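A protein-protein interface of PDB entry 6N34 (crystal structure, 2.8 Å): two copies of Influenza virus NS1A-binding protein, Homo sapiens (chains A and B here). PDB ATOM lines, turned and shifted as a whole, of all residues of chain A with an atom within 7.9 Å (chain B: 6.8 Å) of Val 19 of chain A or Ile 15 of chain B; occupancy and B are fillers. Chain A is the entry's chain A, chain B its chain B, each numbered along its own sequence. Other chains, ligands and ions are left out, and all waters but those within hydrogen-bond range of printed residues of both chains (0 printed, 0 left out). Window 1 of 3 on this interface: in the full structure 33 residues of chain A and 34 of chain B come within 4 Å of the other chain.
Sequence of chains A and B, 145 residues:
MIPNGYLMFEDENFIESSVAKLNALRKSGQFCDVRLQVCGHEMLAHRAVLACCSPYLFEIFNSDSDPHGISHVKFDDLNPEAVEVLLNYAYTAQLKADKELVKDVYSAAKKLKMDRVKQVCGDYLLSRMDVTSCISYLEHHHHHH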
ATOM      1  N   ASN A  13      14.817 -30.360   4.985  1.00  0.00           N
ATOM      2  CA  ASN A  13      14.192 -29.084   4.644  1.00  0.00           C
ATOM      3  C   ASN A  13      13.829 -28.294   5.900  1.00  0.00           C
ATOM      4  O   ASN A  13      13.956 -27.062   5.928  1.00  0.00           O
ATOM      5  CB  ASN A  13      12.942 -29.314   3.788  1.00  0.00           C
ATOM      6  CG  ASN A  13      13.267 -29.516   2.322  1.00  0.00           C
ATOM      7  OD1 ASN A  13      12.758 -30.443   1.680  1.00  0.00           O
ATOM      8  ND2 ASN A  13      14.120 -28.647   1.782  1.00  0.00           N
ATOM      9  N   PHE A  14      13.392 -28.993   6.951  1.00  0.00           N
ATOM     10  CA  PHE A  14      12.792 -28.336   8.108  1.00  0.00           C
ATOM     11  C   PHE A  14      13.721 -27.312   8.757  1.00  0.00           C
ATOM     12  O   PHE A  14      13.241 -26.347   9.365  1.00  0.00           O
ATOM     13  CB  PHE A  14      12.371 -29.388   9.135  1.00  0.00           C
ATOM     14  CG  PHE A  14      11.596 -28.828  10.290  1.00  0.00           C
ATOM     15  CD1 PHE A  14      10.310 -28.345  10.105  1.00  0.00           C
ATOM     16  CD2 PHE A  14      12.150 -28.795  11.558  1.00  0.00           C
ATOM     17  CE1 PHE A  14       9.595 -27.835  11.160  1.00  0.00           C
ATOM     18  CE2 PHE A  14      11.444 -28.292  12.615  1.00  0.00           C
ATOM     19  CZ  PHE A  14      10.165 -27.806  12.421  1.00  0.00           C
ATOM     20  N   ILE A  15      15.038 -27.489   8.647  1.00  0.00           N
ATOM     21  CA  ILE A  15      15.924 -26.585   9.378  1.00  0.00           C
ATOM     22  C   ILE A  15      16.016 -25.234   8.687  1.00  0.00           C
ATOM     23  O   ILE A  15      16.010 -24.189   9.349  1.00  0.00           O
ATOM     24  CB  ILE A  15      17.313 -27.211   9.580  1.00  0.00           C
ATOM     25  CG1 ILE A  15      17.253 -28.330  10.622  1.00  0.00           C
ATOM     26  CG2 ILE A  15      18.311 -26.152  10.012  1.00  0.00           C
ATOM     27  CD1 ILE A  15      16.868 -27.847  12.025  1.00  0.00           C
ATOM     28  N   GLU A  16      16.098 -25.224   7.355  1.00  0.00           N
ATOM     29  CA  GLU A  16      16.172 -23.958   6.634  1.00  0.00           C
ATOM     30  C   GLU A  16      14.821 -23.251   6.566  1.00  0.00           C
ATOM     31  O   GLU A  16      14.782 -22.015   6.554  1.00  0.00           O
ATOM     32  CB  GLU A  16      16.717 -24.179   5.222  1.00  0.00           C
ATOM     33  CG  GLU A  16      18.060 -24.934   5.141  1.00  0.00           C
ATOM     34  CD  GLU A  16      19.285 -24.022   5.193  1.00  0.00           C
ATOM     35  OE1 GLU A  16      19.359 -23.169   6.108  1.00  0.00           O
ATOM     36  OE2 GLU A  16      20.176 -24.172   4.318  1.00  0.00           O
ATOM     37  N   SER A  17      13.713 -24.001   6.547  1.00  0.00           N
ATOM     38  CA  SER A  17      12.396 -23.378   6.457  1.00  0.00           C
ATOM     39  C   SER A  17      11.970 -22.716   7.764  1.00  0.00           C
ATOM     40  O   SER A  17      11.037 -21.904   7.759  1.00  0.00           O
ATOM     41  CB  SER A  17      11.347 -24.409   6.022  1.00  0.00           C
ATOM     42  OG  SER A  17      10.825 -25.147   7.114  1.00  0.00           O
ATOM     43  N   SER A  18      12.629 -23.017   8.879  1.00  0.00           N
ATOM     44  CA  SER A  18      12.184 -22.451  10.140  1.00  0.00           C
ATOM     45  C   SER A  18      13.090 -21.341  10.657  1.00  0.00           C
ATOM     46  O   SER A  18      12.598 -20.459  11.368  1.00  0.00           O
ATOM     47  CB  SER A  18      12.023 -23.553  11.202  1.00  0.00           C
ATOM     48  OG  SER A  18      13.177 -24.365  11.330  1.00  0.00           O
ATOM     49  N   VAL A  19      14.391 -21.342  10.325  1.00  0.00           N
ATOM     50  CA  VAL A  19      15.167 -20.124  10.569  1.00  0.00           C
ATOM     51  C   VAL A  19      14.616 -18.987   9.719  1.00  0.00           C
ATOM     52  O   VAL A  19      14.636 -17.827  10.136  1.00  0.00           O
ATOM     53  CB  VAL A  19      16.686 -20.308  10.321  1.00  0.00           C
ATOM     54  CG1 VAL A  19      17.316 -21.277  11.328  1.00  0.00           C
ATOM     55  CG2 VAL A  19      16.976 -20.721   8.895  1.00  0.00           C
ATOM     56  N   ALA A  20      14.110 -19.300   8.528  1.00  0.00           N
ATOM     57  CA  ALA A  20      13.429 -18.298   7.725  1.00  0.00           C
ATOM     58  C   ALA A  20      12.129 -17.863   8.387  1.00  0.00           C
ATOM     59  O   ALA A  20      11.835 -16.666   8.458  1.00  0.00           O
ATOM     60  CB  ALA A  20      13.173 -18.843   6.322  1.00  0.00           C
ATOM     61  N   LYS A  21      11.398 -18.835   8.901  1.00  0.00           N
ATOM     62  CA  LYS A  21      10.133 -18.491   9.568  1.00  0.00           C
ATOM     63  C   LYS A  21      10.501 -17.709  10.811  1.00  0.00           C
ATOM     64  O   LYS A  21       9.939 -16.664  11.012  1.00  0.00           O
ATOM     65  CB  LYS A  21       9.343 -19.751   9.903  1.00  0.00           C
ATOM     66  CG  LYS A  21       8.809 -20.514   8.706  1.00  0.00           C
ATOM     67  CD  LYS A  21       7.589 -21.332   9.021  1.00  0.00           C
ATOM     68  CE  LYS A  21       7.149 -22.202   7.869  1.00  0.00           C
ATOM     69  NZ  LYS A  21       7.592 -23.602   8.040  1.00  0.00           N
ATOM     70  N   LEU A  22      11.461 -18.191  11.575  1.00  0.00           N
ATOM     71  CA  LEU A  22      11.829 -17.455  12.798  1.00  0.00           C
ATOM     72  C   LEU A  22      12.336 -16.084  12.415  1.00  0.00           C
ATOM     73  O   LEU A  22      11.953 -15.129  13.015  1.00  0.00           O
ATOM     74  CB  LEU A  22      12.913 -18.228  13.525  1.00  0.00           C
ATOM     75  CG  LEU A  22      12.436 -18.750  14.859  1.00  0.00           C
ATOM     76  CD1 LEU A  22      13.313 -19.865  15.339  1.00  0.00           C
ATOM     77  CD2 LEU A  22      12.399 -17.626  15.847  1.00  0.00           C
ATOM     78  N   ASN A  23      13.182 -16.009  11.421  1.00  0.00           N
ATOM     79  CA  ASN A  23      13.667 -14.668  11.062  1.00  0.00           C
ATOM     80  C   ASN A  23      12.456 -13.824  10.706  1.00  0.00           C
ATOM     81  O   ASN A  23      12.355 -12.736  11.205  1.00  0.00           O
ATOM     82  CB  ASN A  23      14.650 -14.752   9.914  1.00  0.00           C
ATOM     83  CG  ASN A  23      15.426 -13.474   9.820  1.00  0.00           C
ATOM     84  OD1 ASN A  23      15.366 -12.663  10.729  1.00  0.00           O
ATOM     85  ND2 ASN A  23      16.128 -13.285   8.727  1.00  0.00           N
ATOM     86  N   ALA A  24      11.571 -14.346   9.869  1.00  0.00           N
ATOM     87  CA  ALA A  24      10.337 -13.663   9.499  1.00  0.00           C
ATOM     88  C   ALA A  24       9.594 -13.147  10.735  1.00  0.00           C
ATOM     89  O   ALA A  24       9.111 -12.007  10.752  1.00  0.00           O
ATOM     90  CB  ALA A  24       9.454 -14.601   8.683  1.00  0.00           C
ATOM     91  N   LEU A  25       9.511 -13.975  11.788  1.00  0.00           N
ATOM     92  CA  LEU A  25       8.851 -13.567  13.032  1.00  0.00           C
ATOM     93  C   LEU A  25       9.502 -12.330  13.634  1.00  0.00           C
ATOM     94  O   LEU A  25       8.817 -11.353  13.968  1.00  0.00           O
ATOM     95  CB  LEU A  25       8.886 -14.699  14.054  1.00  0.00           C
ATOM     96  CG  LEU A  25       7.843 -15.789  13.842  1.00  0.00           C
ATOM     97  CD1 LEU A  25       7.728 -16.658  15.089  1.00  0.00           C
ATOM     98  CD2 LEU A  25       6.497 -15.171  13.447  1.00  0.00           C
ATOM     99  N   ARG A  26      10.829 -12.370  13.802  1.00  0.00           N
ATOM    100  CA  ARG A  26      11.541 -11.248  14.400  1.00  0.00           C
ATOM    101  C   ARG A  26      11.301  -9.959  13.622  1.00  0.00           C
ATOM    102  O   ARG A  26      11.015  -8.917  14.218  1.00  0.00           O
ATOM    103  CB  ARG A  26      13.030 -11.564  14.488  1.00  0.00           C
ATOM    104  CG  ARG A  26      13.844 -10.451  15.114  1.00  0.00           C
ATOM    105  CD  ARG A  26      15.335 -10.675  14.945  1.00  0.00           C
ATOM    106  NE  ARG A  26      15.699 -10.826  13.542  1.00  0.00           N
ATOM    107  CZ  ARG A  26      16.292  -9.878  12.832  1.00  0.00           C
ATOM    108  NH1 ARG A  26      16.599  -8.720  13.414  1.00  0.00           N
ATOM    109  NH2 ARG A  26      16.582 -10.089  11.551  1.00  0.00           N
ATOM    110  N   ASN A  88      20.833 -10.559  12.469  1.00  0.00           N
ATOM    111  CA  ASN A  88      20.556 -11.447  11.353  1.00  0.00           C
ATOM    112  C   ASN A  88      21.372 -12.716  11.476  1.00  0.00           C
ATOM    113  O   ASN A  88      20.914 -13.807  11.123  1.00  0.00           O
ATOM    114  CB  ASN A  88      20.840 -10.740  10.035  1.00  0.00           C
ATOM    115  CG  ASN A  88      19.598 -10.130   9.442  1.00  0.00           C
ATOM    116  OD1 ASN A  88      18.527 -10.731   9.503  1.00  0.00           O
ATOM    117  ND2 ASN A  88      19.719  -8.919   8.884  1.00  0.00           N
ATOM    118  N   TYR A  89      22.572 -12.597  12.020  1.00  0.00           N
ATOM    119  CA  TYR A  89      23.437 -13.755  12.073  1.00  0.00           C
ATOM    120  C   TYR A  89      22.991 -14.704  13.177  1.00  0.00           C
ATOM    121  O   TYR A  89      23.041 -15.932  13.012  1.00  0.00           O
ATOM    122  CB  TYR A  89      24.881 -13.286  12.233  1.00  0.00           C
ATOM    123  CG  TYR A  89      25.802 -14.305  12.807  1.00  0.00           C
ATOM    124  CD1 TYR A  89      25.944 -14.410  14.179  1.00  0.00           C
ATOM    125  CD2 TYR A  89      26.527 -15.178  11.990  1.00  0.00           C
ATOM    126  CE1 TYR A  89      26.766 -15.352  14.734  1.00  0.00           C
ATOM    127  CE2 TYR A  89      27.376 -16.130  12.550  1.00  0.00           C
ATOM    128  CZ  TYR A  89      27.487 -16.200  13.933  1.00  0.00           C
ATOM    129  OH  TYR A  89      28.315 -17.090  14.554  1.00  0.00           O
ATOM    130  N   ALA A  90      22.526 -14.161  14.302  1.00  0.00           N
ATOM    131  CA  ALA A  90      21.989 -15.018  15.358  1.00  0.00           C
ATOM    132  C   ALA A  90      20.793 -15.821  14.880  1.00  0.00           C
ATOM    133  O   ALA A  90      20.564 -16.933  15.357  1.00  0.00           O
ATOM    134  CB  ALA A  90      21.594 -14.190  16.575  1.00  0.00           C
ATOM    135  N   TYR A  91      20.022 -15.286  13.950  1.00  0.00           N
ATOM    136  CA  TYR A  91      18.854 -16.018  13.499  1.00  0.00           C
ATOM    137  C   TYR A  91      19.194 -16.984  12.380  1.00  0.00           C
ATOM    138  O   TYR A  91      18.884 -18.176  12.474  1.00  0.00           O
ATOM    139  CB  TYR A  91      17.756 -15.043  13.069  1.00  0.00           C
ATOM    140  CG  TYR A  91      16.926 -14.641  14.250  1.00  0.00           C
ATOM    141  CD1 TYR A  91      17.425 -13.753  15.189  1.00  0.00           C
ATOM    142  CD2 TYR A  91      15.682 -15.199  14.468  1.00  0.00           C
ATOM    143  CE1 TYR A  91      16.697 -13.403  16.303  1.00  0.00           C
ATOM    144  CE2 TYR A  91      14.942 -14.854  15.569  1.00  0.00           C
ATOM    145  CZ  TYR A  91      15.450 -13.954  16.489  1.00  0.00           C
ATOM    146  OH  TYR A  91      14.707 -13.611  17.589  1.00  0.00           O
ATOM    147  N   THR A  92      19.888 -16.489  11.361  1.00  0.00           N
ATOM    148  CA  THR A  92      20.089 -17.178  10.098  1.00  0.00           C
ATOM    149  C   THR A  92      21.450 -17.828   9.960  1.00  0.00           C
ATOM    150  O   THR A  92      21.698 -18.472   8.934  1.00  0.00           O
ATOM    151  CB  THR A  92      19.921 -16.192   8.942  1.00  0.00           C
ATOM    152  OG1 THR A  92      21.137 -15.452   8.759  1.00  0.00           O
ATOM    153  CG2 THR A  92      18.798 -15.236   9.244  1.00  0.00           C
ATOM    154  N   ALA A  93      22.345 -17.637  10.928  1.00  0.00           N
ATOM    155  CA  ALA A  93      23.742 -18.071  10.884  1.00  0.00           C
ATOM    156  C   ALA A  93      24.550 -17.394   9.786  1.00  0.00           C
ATOM    157  O   ALA A  93      25.658 -17.860   9.477  1.00  0.00           O
ATOM    158  CB  ALA A  93      23.879 -19.584  10.725  1.00  0.00           C
ATOM    159  N   GLN A  94      24.051 -16.310   9.192  1.00  0.00           N
ATOM    160  CA  GLN A  94      24.731 -15.632   8.095  1.00  0.00           C
ATOM    161  C   GLN A  94      25.164 -14.225   8.492  1.00  0.00           C
ATOM    162  O   GLN A  94      24.373 -13.445   9.037  1.00  0.00           O
ATOM    163  CB  GLN A  94      23.851 -15.572   6.848  1.00  0.00           C
ATOM    164  CG  GLN A  94      24.008 -16.783   5.963  1.00  0.00           C
ATOM    165  CD  GLN A  94      23.306 -16.620   4.626  1.00  0.00           C
ATOM    166  OE1 GLN A  94      23.058 -15.500   4.171  1.00  0.00           O
ATOM    167  NE2 GLN A  94      22.988 -17.738   3.983  1.00  0.00           N
ATOM    168  N   GLU B  10      29.311 -17.396   6.279  1.00  0.00           N
ATOM    169  CA  GLU B  10      28.305 -18.282   6.834  1.00  0.00           C
ATOM    170  C   GLU B  10      28.968 -19.237   7.815  1.00  0.00           C
ATOM    171  O   GLU B  10      30.033 -19.790   7.534  1.00  0.00           O
ATOM    172  CB  GLU B  10      27.583 -19.057   5.738  1.00  0.00           C
ATOM    173  CG  GLU B  10      26.637 -20.111   6.271  1.00  0.00           C
ATOM    174  CD  GLU B  10      25.410 -20.308   5.391  1.00  0.00           C
ATOM    175  OE1 GLU B  10      25.554 -20.665   4.195  1.00  0.00           O
ATOM    176  OE2 GLU B  10      24.288 -20.100   5.907  1.00  0.00           O
ATOM    177  N   ASP B  11      28.351 -19.404   8.976  1.00  0.00           N
ATOM    178  CA  ASP B  11      28.885 -20.277  10.013  1.00  0.00           C
ATOM    179  C   ASP B  11      28.191 -21.628   9.888  1.00  0.00           C
ATOM    180  O   ASP B  11      27.106 -21.835  10.438  1.00  0.00           O
ATOM    181  CB  ASP B  11      28.684 -19.661  11.388  1.00  0.00           C
ATOM    182  CG  ASP B  11      29.564 -20.296  12.425  1.00  0.00           C
ATOM    183  OD1 ASP B  11      30.370 -21.172  12.044  1.00  0.00           O
ATOM    184  OD2 ASP B  11      29.462 -19.922  13.613  1.00  0.00           O
ATOM    185  N   GLU B  12      28.829 -22.553   9.161  1.00  0.00           N
ATOM    186  CA  GLU B  12      28.220 -23.852   8.889  1.00  0.00           C
ATOM    187  C   GLU B  12      28.048 -24.687  10.151  1.00  0.00           C
ATOM    188  O   GLU B  12      27.350 -25.705  10.117  1.00  0.00           O
ATOM    189  CB  GLU B  12      29.049 -24.617   7.846  1.00  0.00           C
ATOM    190  CG  GLU B  12      28.355 -25.837   7.232  1.00  0.00           C
ATOM    191  CD  GLU B  12      26.977 -25.514   6.665  1.00  0.00           C
ATOM    192  OE1 GLU B  12      26.781 -24.388   6.159  1.00  0.00           O
ATOM    193  OE2 GLU B  12      26.083 -26.385   6.730  1.00  0.00           O
ATOM    194  N   ASN B  13      28.665 -24.282  11.256  1.00  0.00           N
ATOM    195  CA  ASN B  13      28.463 -24.946  12.534  1.00  0.00           C
ATOM    196  C   ASN B  13      27.400 -24.280  13.387  1.00  0.00           C
ATOM    197  O   ASN B  13      26.757 -24.963  14.192  1.00  0.00           O
ATOM    198  CB  ASN B  13      29.769 -24.977  13.322  1.00  0.00           C
ATOM    199  CG  ASN B  13      30.727 -26.026  12.812  1.00  0.00           C
ATOM    200  OD1 ASN B  13      30.335 -27.159  12.545  1.00  0.00           O
ATOM    201  ND2 ASN B  13      31.991 -25.649  12.656  1.00  0.00           N
ATOM    202  N   PHE B  14      27.192 -22.972  13.220  1.00  0.00           N
ATOM    203  CA  PHE B  14      26.348 -22.224  14.151  1.00  0.00           C
ATOM    204  C   PHE B  14      24.955 -22.821  14.250  1.00  0.00           C
ATOM    205  O   PHE B  14      24.405 -22.944  15.351  1.00  0.00           O
ATOM    206  CB  PHE B  14      26.253 -20.747  13.746  1.00  0.00           C
ATOM    207  CG  PHE B  14      25.333 -19.938  14.626  1.00  0.00           C
ATOM    208  CD1 PHE B  14      25.720 -19.574  15.909  1.00  0.00           C
ATOM    209  CD2 PHE B  14      24.073 -19.565  14.177  1.00  0.00           C
ATOM    210  CE1 PHE B  14      24.871 -18.851  16.729  1.00  0.00           C
ATOM    211  CE2 PHE B  14      23.225 -18.840  14.985  1.00  0.00           C
ATOM    212  CZ  PHE B  14      23.626 -18.482  16.268  1.00  0.00           C
ATOM    213  N   ILE B  15      24.376 -23.219  13.119  1.00  0.00           N
ATOM    214  CA  ILE B  15      22.998 -23.696  13.145  1.00  0.00           C
ATOM    215  C   ILE B  15      22.880 -24.948  14.013  1.00  0.00           C
ATOM    216  O   ILE B  15      22.098 -24.972  14.967  1.00  0.00           O
ATOM    217  CB  ILE B  15      22.471 -23.907  11.713  1.00  0.00           C
ATOM    218  CG1 ILE B  15      21.994 -22.572  11.119  1.00  0.00           C
ATOM    219  CG2 ILE B  15      21.339 -24.903  11.680  1.00  0.00           C
ATOM    220  CD1 ILE B  15      21.187 -21.670  12.090  1.00  0.00           C
ATOM    221  N   GLU B  16      23.689 -25.985  13.741  1.00  0.00           N
ATOM    222  CA  GLU B  16      23.500 -27.250  14.459  1.00  0.00           C
ATOM    223  C   GLU B  16      23.872 -27.152  15.932  1.00  0.00           C
ATOM    224  O   GLU B  16      23.264 -27.835  16.768  1.00  0.00           O
ATOM    225  CB  GLU B  16      24.288 -28.390  13.814  1.00  0.00           C
ATOM    226  CG  GLU B  16      25.776 -28.194  13.662  1.00  0.00           C
ATOM    227  CD  GLU B  16      26.140 -27.950  12.215  1.00  0.00           C
ATOM    228  OE1 GLU B  16      25.649 -26.928  11.679  1.00  0.00           O
ATOM    229  OE2 GLU B  16      26.860 -28.788  11.612  1.00  0.00           O
ATOM    230  N   SER B  17      24.863 -26.337  16.274  1.00  0.00           N
ATOM    231  CA  SER B  17      25.150 -26.112  17.685  1.00  0.00           C
ATOM    232  C   SER B  17      24.030 -25.326  18.364  1.00  0.00           C
ATOM    233  O   SER B  17      23.702 -25.579  19.530  1.00  0.00           O
ATOM    234  CB  SER B  17      26.482 -25.387  17.824  1.00  0.00           C
ATOM    235  OG  SER B  17      26.517 -24.253  16.970  1.00  0.00           O
ATOM    236  N   SER B  18      23.421 -24.374  17.650  1.00  0.00           N
ATOM    237  CA  SER B  18      22.428 -23.524  18.296  1.00  0.00           C
ATOM    238  C   SER B  18      21.123 -24.284  18.554  1.00  0.00           C
ATOM    239  O   SER B  18      20.471 -24.056  19.582  1.00  0.00           O
ATOM    240  CB  SER B  18      22.222 -22.236  17.470  1.00  0.00           C
ATOM    241  OG  SER B  18      21.102 -22.279  16.599  1.00  0.00           O
ATOM    242  N   VAL B  19      20.744 -25.219  17.675  1.00  0.00           N
ATOM    243  CA  VAL B  19      19.539 -26.010  17.931  1.00  0.00           C
ATOM    244  C   VAL B  19      19.740 -26.921  19.137  1.00  0.00           C
ATOM    245  O   VAL B  19      18.804 -27.167  19.906  1.00  0.00           O
ATOM    246  CB  VAL B  19      19.122 -26.804  16.675  1.00  0.00           C
ATOM    247  CG1 VAL B  19      19.109 -25.897  15.446  1.00  0.00           C
ATOM    248  CG2 VAL B  19      20.004 -28.055  16.451  1.00  0.00           C
ATOM    249  N   ALA B  20      20.959 -27.439  19.322  1.00  0.00           N
ATOM    250  CA  ALA B  20      21.260 -28.205  20.522  1.00  0.00           C
ATOM    251  C   ALA B  20      21.010 -27.372  21.771  1.00  0.00           C
ATOM    252  O   ALA B  20      20.434 -27.859  22.750  1.00  0.00           O
ATOM    253  CB  ALA B  20      22.707 -28.699  20.477  1.00  0.00           C
ATOM    254  N   CYS B  52       6.489 -21.817  14.209  1.00  0.00           N
ATOM    255  CA  CYS B  52       7.078 -22.221  12.930  1.00  0.00           C
ATOM    256  C   CYS B  52       6.752 -23.665  12.575  1.00  0.00           C
ATOM    257  O   CYS B  52       6.719 -24.023  11.391  1.00  0.00           O
ATOM    258  CB  CYS B  52       8.601 -22.069  12.952  1.00  0.00           C
ATOM    259  SG  CYS B  52       9.196 -20.538  13.628  1.00  0.00           S
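Printed residues of chain B that touch a printed residue of chain A: Glu 10, Asp 11, Phe 14, Ile 15 and Cys 52.
Hydrophobic or aromatic side chains of chain B within 4 Å of the printed part of chain A: Phe 14 and Ile 15.
Along chain B the printed residues that touch a printed residue of chain A span positions 10 to 52.
Hydrophobic or aromatic side chains of chain A that line the printed part of chain B: Ile 15, Val 19, Leu 22, Tyr 89 and Ala 93.
Among the printed residues, no Asp or Glu carboxylate lies within 4 Å of a Lys or Arg side-chain nitrogen of the other chain.
Ile 15 of chain A touches its own counterpart, Ile 15 of chain B.
Val 19 of chain A touches Ile 15 of chain B, but with the chains exchanged Ile 15 of chain A does not touch Val 19 of chain B (4.5 Å).
8 positions are printed for both chains.
Of the 12 pairs that touch across the chains among the printed residues, 1 has its exchanged pair printed and touching as well.
Among the printed residues, pairs that only touch across the chains: Ala 90 of chain A with Phe 14 of chain B (3.3 Å), Ala 93 of chain A with Phe 14 of chain B (3.5 Å), Tyr 89 of chain A with Phe 14 of chain B (3.5 Å), Ala 93 of chain A with Ile 15 of chain B (3.6 Å), Ile 15 of chain A with Ile 15 of chain B (3.7 Å), Ala 93 of chain A with Glu 10 of chain B (3.8 Å), Leu 22 of chain A with Cys 52 of chain B (3.9 Å) and Val 19 of chain A with Ile 15 of chain B (3.96 Å).
The side-chain carboxylate (OE2) of Glu 10 of chain B is in hydrogen-bond range of the side-chain amide nitrogen (NE2) of Gln 94 of chain A, at 3.3 Å.
The backbone carbonyl oxygen of Cys 52 of chain B lies within hydrogen-bond range of the side-chain amino group of Lys 21 of chain A, at 3.5 Å.
The backbone NH (N) of Asp 11 of chain B lies within hydrogen-bond range of the backbone carbonyl oxygen (O) of Ala 93 of chain A.
The side-chain carboxylate (OD2) of Asp 11 of chain B lies within hydrogen-bond range of the side-chain hydroxyl (OH) of Tyr 89 of chain A (3.2 Å).
Printed residues of chain B within 4 Å of Val 19 of chain A: Ile 15.
Of the printed residues of chain B, Leu 22 of chain A touches Cys 52.
Of the printed residues of chain B, Ala 93 of chain A touches Glu 10, Asp 11, Phe 14 and Ile 15.
Printed residues of chain B within 4 Å of Gln 94 of chain A: Glu 10 (3.3 Å).
Of chain A, only Ile 15 (3.7 Å), Val 19 (3.96 Å) and Ala 93 (3.6 Å) come within 4 Å of Ile 15 of chain B.
The nearest residue of chain B that does not touch Val 19 of chain A is Cys 52 of chain B (6.2 Å).
The nearest residue of chain A that does not touch Ile 15 of chain B is Tyr 91 of chain A (4.2 Å).
O of Phe 14 of chain B lies within hydrogen-bond range of OG of Ser 17 of chain B (3.0 Å).
The side-chain hydroxyl (OG1) of Thr 92 of chain A is in hydrogen-bond range of the backbone NH (N) of Gln 94 of chain A, at 3.1 Å.
The backbone carbonyl oxygen of Ile 15 of chain B lies within hydrogen-bond range of the side-chain hydroxyl of Ser 18 of chain B (3.3 Å).
The backbone carbonyl oxygen (O) of Ile 15 of chain A is in hydrogen-bond range of the side-chain hydroxyl (OG) of Ser 18 of chain A, 3.5 Å away.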
